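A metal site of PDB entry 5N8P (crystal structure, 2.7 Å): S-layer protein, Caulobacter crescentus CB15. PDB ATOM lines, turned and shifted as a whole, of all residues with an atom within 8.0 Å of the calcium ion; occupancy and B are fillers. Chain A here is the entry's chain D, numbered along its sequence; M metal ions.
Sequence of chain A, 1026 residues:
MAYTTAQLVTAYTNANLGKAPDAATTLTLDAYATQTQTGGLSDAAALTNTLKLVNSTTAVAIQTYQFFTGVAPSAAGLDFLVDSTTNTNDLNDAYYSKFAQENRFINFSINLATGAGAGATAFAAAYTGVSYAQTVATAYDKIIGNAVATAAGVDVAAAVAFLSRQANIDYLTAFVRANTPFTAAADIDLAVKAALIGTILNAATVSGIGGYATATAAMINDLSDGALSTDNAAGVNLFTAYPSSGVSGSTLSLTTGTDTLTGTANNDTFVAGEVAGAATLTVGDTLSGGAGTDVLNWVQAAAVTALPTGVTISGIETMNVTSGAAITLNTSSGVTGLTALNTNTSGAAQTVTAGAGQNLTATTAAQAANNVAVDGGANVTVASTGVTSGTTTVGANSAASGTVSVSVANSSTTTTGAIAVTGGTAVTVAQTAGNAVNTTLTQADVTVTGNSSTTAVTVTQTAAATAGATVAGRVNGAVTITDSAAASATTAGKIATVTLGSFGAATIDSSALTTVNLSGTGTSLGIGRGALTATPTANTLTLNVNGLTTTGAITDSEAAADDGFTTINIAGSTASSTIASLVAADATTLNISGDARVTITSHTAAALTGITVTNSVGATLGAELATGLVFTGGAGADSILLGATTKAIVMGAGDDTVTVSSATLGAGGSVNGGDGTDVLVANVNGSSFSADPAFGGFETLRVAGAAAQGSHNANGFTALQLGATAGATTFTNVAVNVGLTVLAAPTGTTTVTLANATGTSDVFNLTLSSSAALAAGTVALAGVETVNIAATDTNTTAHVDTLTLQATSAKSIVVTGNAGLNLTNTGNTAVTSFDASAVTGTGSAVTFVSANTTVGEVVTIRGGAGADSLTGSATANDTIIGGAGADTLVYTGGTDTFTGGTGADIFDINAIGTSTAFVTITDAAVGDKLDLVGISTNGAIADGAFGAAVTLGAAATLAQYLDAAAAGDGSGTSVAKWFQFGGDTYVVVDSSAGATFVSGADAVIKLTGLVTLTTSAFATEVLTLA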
ATOM      1  N   LEU A 962      -0.267  -5.375   3.241  1.00  0.00           N
ATOM      2  CA  LEU A 962      -1.021  -6.654   3.197  1.00  0.00           C
ATOM      3  C   LEU A 962      -2.272  -6.554   4.068  1.00  0.00           C
ATOM      4  O   LEU A 962      -3.395  -6.695   3.574  1.00  0.00           O
ATOM      5  CB  LEU A 962      -0.140  -7.849   3.615  1.00  0.00           C
ATOM      6  CG  LEU A 962       0.926  -8.343   2.623  1.00  0.00           C
ATOM      7  CD1 LEU A 962       2.034  -9.124   3.313  1.00  0.00           C
ATOM      8  CD2 LEU A 962       0.325  -9.166   1.480  1.00  0.00           C
ATOM      9  N   ASP A 963      -2.049  -6.280   5.354  1.00  0.00           N
ATOM     10  CA  ASP A 963      -3.125  -6.004   6.328  1.00  0.00           C
ATOM     11  C   ASP A 963      -4.162  -4.980   5.823  1.00  0.00           C
ATOM     12  O   ASP A 963      -5.372  -5.190   5.960  1.00  0.00           O
ATOM     13  CB  ASP A 963      -2.521  -5.546   7.680  1.00  0.00           C
ATOM     14  CG  ASP A 963      -1.937  -6.686   8.492  1.00  0.00           C
ATOM     15  OD1 ASP A 963      -2.463  -7.842   8.467  1.00  0.00           O
ATOM     16  OD2 ASP A 963      -0.938  -6.365   9.166  1.00  0.00           O
ATOM     17  N   ALA A 964      -3.679  -3.893   5.225  1.00  0.00           N
ATOM     18  CA  ALA A 964      -4.544  -2.870   4.620  1.00  0.00           C
ATOM     19  C   ALA A 964      -5.418  -3.479   3.522  1.00  0.00           C
ATOM     20  O   ALA A 964      -6.633  -3.261   3.518  1.00  0.00           O
ATOM     21  CB  ALA A 964      -3.738  -1.693   4.112  1.00  0.00           C
ATOM     22  N   ALA A 965      -4.801  -4.278   2.636  1.00  0.00           N
ATOM     23  CA  ALA A 965      -5.474  -4.899   1.494  1.00  0.00           C
ATOM     24  C   ALA A 965      -6.519  -5.923   1.903  1.00  0.00           C
ATOM     25  O   ALA A 965      -7.540  -6.075   1.253  1.00  0.00           O
ATOM     26  CB  ALA A 965      -4.458  -5.532   0.553  1.00  0.00           C
ATOM     27  N   ALA A 966      -6.271  -6.602   3.021  1.00  0.00           N
ATOM     28  CA  ALA A 966      -7.169  -7.629   3.508  1.00  0.00           C
ATOM     29  C   ALA A 966      -8.138  -7.105   4.555  1.00  0.00           C
ATOM     30  O   ALA A 966      -8.798  -7.915   5.225  1.00  0.00           O
ATOM     31  CB  ALA A 966      -6.382  -8.798   4.066  1.00  0.00           C
ATOM     32  N   ALA A 967      -8.229  -5.790   4.716  1.00  0.00           N
ATOM     33  CA  ALA A 967      -9.033  -5.188   5.806  1.00  0.00           C
ATOM     34  C   ALA A 967     -10.493  -5.647   5.816  1.00  0.00           C
ATOM     35  O   ALA A 967     -11.034  -5.940   6.895  1.00  0.00           O
ATOM     36  CB  ALA A 967      -8.932  -3.660   5.811  1.00  0.00           C
ATOM     37  N   GLY A 968     -11.091  -5.744   4.612  1.00  0.00           N
ATOM     38  CA  GLY A 968     -12.495  -6.129   4.423  1.00  0.00           C
ATOM     39  C   GLY A 968     -12.891  -7.526   4.882  1.00  0.00           C
ATOM     40  O   GLY A 968     -12.064  -8.300   5.419  1.00  0.00           O
ATOM     41  N   ASP A 969     -14.168  -7.846   4.661  1.00  0.00           N
ATOM     42  CA  ASP A 969     -14.694  -9.167   5.019  1.00  0.00           C
ATOM     43  C   ASP A 969     -14.837 -10.106   3.820  1.00  0.00           C
ATOM     44  O   ASP A 969     -15.676  -9.892   2.926  1.00  0.00           O
ATOM     45  CB  ASP A 969     -16.042  -9.041   5.744  1.00  0.00           C
ATOM     46  CG  ASP A 969     -16.478 -10.354   6.383  1.00  0.00           C
ATOM     47  OD1 ASP A 969     -17.686 -10.649   6.364  1.00  0.00           O
ATOM     48  OD2 ASP A 969     -15.599 -11.100   6.881  1.00  0.00           O
ATOM     49  N   GLY A 970     -14.002 -11.160   3.842  1.00  0.00           N
ATOM     50  CA  GLY A 970     -13.976 -12.187   2.790  1.00  0.00           C
ATOM     51  C   GLY A 970     -14.597 -13.516   3.164  1.00  0.00           C
ATOM     52  O   GLY A 970     -14.401 -14.509   2.462  1.00  0.00           O
ATOM     53  N   SER A 971     -15.365 -13.527   4.262  1.00  0.00           N
ATOM     54  CA  SER A 971     -15.994 -14.740   4.816  1.00  0.00           C
ATOM     55  C   SER A 971     -17.078 -15.343   3.936  1.00  0.00           C
ATOM     56  O   SER A 971     -17.185 -16.572   3.841  1.00  0.00           O
ATOM     57  CB  SER A 971     -16.582 -14.466   6.210  1.00  0.00           C
ATOM     58  OG  SER A 971     -15.549 -14.265   7.151  1.00  0.00           O
ATOM     59  N   VAL A 975     -12.466 -11.220  -2.075  1.00  0.00           N
ATOM     60  CA  VAL A 975     -12.245  -9.972  -2.821  1.00  0.00           C
ATOM     61  C   VAL A 975     -10.802  -9.788  -3.226  1.00  0.00           C
ATOM     62  O   VAL A 975      -9.899 -10.182  -2.497  1.00  0.00           O
ATOM     63  CB  VAL A 975     -12.776  -8.672  -2.113  1.00  0.00           C
ATOM     64  CG1 VAL A 975     -13.264  -7.676  -3.194  1.00  0.00           C
ATOM     65  CG2 VAL A 975     -13.897  -8.979  -1.094  1.00  0.00           C
ATOM     66  N   VAL A 989      -5.915 -11.732  -2.437  1.00  0.00           N
ATOM     67  CA  VAL A 989      -7.275 -12.279  -2.302  1.00  0.00           C
ATOM     68  C   VAL A 989      -7.587 -12.369  -0.809  1.00  0.00           C
ATOM     69  O   VAL A 989      -6.904 -13.080  -0.060  1.00  0.00           O
ATOM     70  CB  VAL A 989      -7.495 -13.646  -3.031  1.00  0.00           C
ATOM     71  CG1 VAL A 989      -8.866 -14.230  -2.736  1.00  0.00           C
ATOM     72  CG2 VAL A 989      -7.323 -13.502  -4.535  1.00  0.00           C
ATOM     73  N   ASP A 990      -8.600 -11.626  -0.392  1.00  0.00           N
ATOM     74  CA  ASP A 990      -9.061 -11.646   0.986  1.00  0.00           C
ATOM     75  C   ASP A 990     -10.196 -12.644   1.087  1.00  0.00           C
ATOM     76  O   ASP A 990     -11.233 -12.493   0.421  1.00  0.00           O
ATOM     77  CB  ASP A 990      -9.502 -10.256   1.436  1.00  0.00           C
ATOM     78  CG  ASP A 990      -9.793 -10.172   2.959  1.00  0.00           C
ATOM     79  OD1 ASP A 990      -9.644 -11.176   3.691  1.00  0.00           O
ATOM     80  OD2 ASP A 990     -10.182  -9.068   3.413  1.00  0.00           O
ATOM     81  N   SER A 991      -9.969 -13.667   1.899  1.00  0.00           N
ATOM     82  CA  SER A 991     -10.967 -14.689   2.169  1.00  0.00           C
ATOM     83  C   SER A 991     -11.301 -14.768   3.660  1.00  0.00           C
ATOM     84  O   SER A 991     -11.861 -15.769   4.123  1.00  0.00           O
ATOM     85  CB  SER A 991     -10.499 -16.046   1.601  1.00  0.00           C
ATOM     86  OG  SER A 991     -10.413 -16.022   0.180  1.00  0.00           O
ATOM     87  N   SER A 992     -10.994 -13.705   4.408  1.00  0.00           N
ATOM     88  CA  SER A 992     -11.095 -13.712   5.870  1.00  0.00           C
ATOM     89  C   SER A 992     -11.906 -12.565   6.533  1.00  0.00           C
ATOM     90  O   SER A 992     -12.214 -11.532   5.886  1.00  0.00           O
ATOM     91  CB  SER A 992      -9.685 -13.811   6.490  1.00  0.00           C
ATOM     92  OG  SER A 992      -9.030 -14.992   6.044  1.00  0.00           O
ATOM     93  N   ALA A 993     -12.245 -12.781   7.800  1.00  0.00           N
ATOM     94  CA  ALA A 993     -12.913 -11.810   8.665  1.00  0.00           C
ATOM     95  C   ALA A 993     -12.060 -10.547   8.890  1.00  0.00           C
ATOM     96  O   ALA A 993     -12.160  -9.588   8.098  1.00  0.00           O
ATOM     97  CB  ALA A 993     -13.301 -12.461  10.003  1.00  0.00           C
ATOM     98  N   GLY A 994     -11.210 -10.580   9.935  1.00  0.00           N
ATOM     99  CA  GLY A 994     -10.447  -9.432  10.433  1.00  0.00           C
ATOM    100  C   GLY A 994      -9.526  -8.726   9.455  1.00  0.00           C
ATOM    101  O   GLY A 994      -9.285  -9.231   8.364  1.00  0.00           O
ATOM    102  N   ALA A 995      -9.016  -7.565   9.850  1.00  0.00           N
ATOM    103  CA  ALA A 995      -8.086  -6.794   9.022  1.00  0.00           C
ATOM    104  C   ALA A 995      -6.644  -7.335   9.028  1.00  0.00           C
ATOM    105  O   ALA A 995      -5.740  -6.682   8.529  1.00  0.00           O
ATOM    106  CB  ALA A 995      -8.123  -5.298   9.380  1.00  0.00           C
ATOM    107  N   THR A 996      -6.438  -8.525   9.601  1.00  0.00           N
ATOM    108  CA  THR A 996      -5.180  -9.245   9.422  1.00  0.00           C
ATOM    109  C   THR A 996      -5.245 -10.052   8.124  1.00  0.00           C
ATOM    110  O   THR A 996      -6.206 -10.800   7.865  1.00  0.00           O
ATOM    111  CB  THR A 996      -4.824 -10.166  10.618  1.00  0.00           C
ATOM    112  OG1 THR A 996      -5.027  -9.444  11.835  1.00  0.00           O
ATOM    113  CG2 THR A 996      -3.370 -10.703  10.539  1.00  0.00           C
ATOM    114  N   PHE A 997      -4.217  -9.857   7.291  1.00  0.00           N
ATOM    115  CA  PHE A 997      -3.892 -10.789   6.231  1.00  0.00           C
ATOM    116  C   PHE A 997      -3.473 -12.063   6.939  1.00  0.00           C
ATOM    117  O   PHE A 997      -2.437 -12.074   7.606  1.00  0.00           O
ATOM    118  CB  PHE A 997      -2.751 -10.232   5.391  1.00  0.00           C
ATOM    119  CG  PHE A 997      -2.396 -11.095   4.215  1.00  0.00           C
ATOM    120  CD1 PHE A 997      -2.721 -10.690   2.933  1.00  0.00           C
ATOM    121  CD2 PHE A 997      -1.741 -12.318   4.374  1.00  0.00           C
ATOM    122  CE1 PHE A 997      -2.413 -11.479   1.832  1.00  0.00           C
ATOM    123  CE2 PHE A 997      -1.427 -13.119   3.290  1.00  0.00           C
ATOM    124  CZ  PHE A 997      -1.762 -12.695   2.013  1.00  0.00           C
ATOM    125  N   VAL A 998      -4.290 -13.110   6.858  1.00  0.00           N
ATOM    126  CA  VAL A 998      -3.892 -14.403   7.468  1.00  0.00           C
ATOM    127  C   VAL A 998      -3.168 -15.304   6.463  1.00  0.00           C
ATOM    128  O   VAL A 998      -3.729 -15.638   5.426  1.00  0.00           O
ATOM    129  CB  VAL A 998      -5.026 -15.142   8.248  1.00  0.00           C
ATOM    130  CG1 VAL A 998      -5.307 -14.453   9.587  1.00  0.00           C
ATOM    131  CG2 VAL A 998      -6.309 -15.272   7.447  1.00  0.00           C
ATOM    132  N   ASP A1002      -5.735 -16.232   3.164  1.00  0.00           N
ATOM    133  CA  ASP A1002      -5.559 -15.047   2.321  1.00  0.00           C
ATOM    134  C   ASP A1002      -4.311 -15.254   1.456  1.00  0.00           C
ATOM    135  O   ASP A1002      -3.345 -15.914   1.882  1.00  0.00           O
ATOM    136  CB  ASP A1002      -5.403 -13.765   3.160  1.00  0.00           C
ATOM    137  CG  ASP A1002      -6.625 -13.444   4.017  1.00  0.00           C
ATOM    138  OD1 ASP A1002      -7.776 -13.751   3.597  1.00  0.00           O
ATOM    139  OD2 ASP A1002      -6.429 -12.858   5.105  1.00  0.00           O
HETATM  140 CA    CA M   1     -10.229  -9.696   5.946  1.00  0.00          CA
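N of Asp 990 sits at hydrogen-bond distance from O of Val 975, 2.9 Å away.
The backbone carbonyl oxygen of Ser 992 sits close to the backbone NH of Gly 970 (2.7 Å).
The side-chain carboxylate of Asp 1002 sits at hydrogen-bond distance from the side-chain hydroxyl of Ser 992 (3.0 Å).
Ala 967 touches the calcium ion (O to CA, 3.96 Å).
The calcium ion is bound by O of Gly 968 (2.4 Å), O of Ala 966 (2.4 Å), OD2 of Asp 990 (2.6 Å), O of Gly 994 (2.6 Å), O of Ser 992 (2.7 Å), OD1 of Asp 990 (2.8 Å) and O of Ala 993 (2.9 Å).
The calcium ion has seven donor atoms within binding distance.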
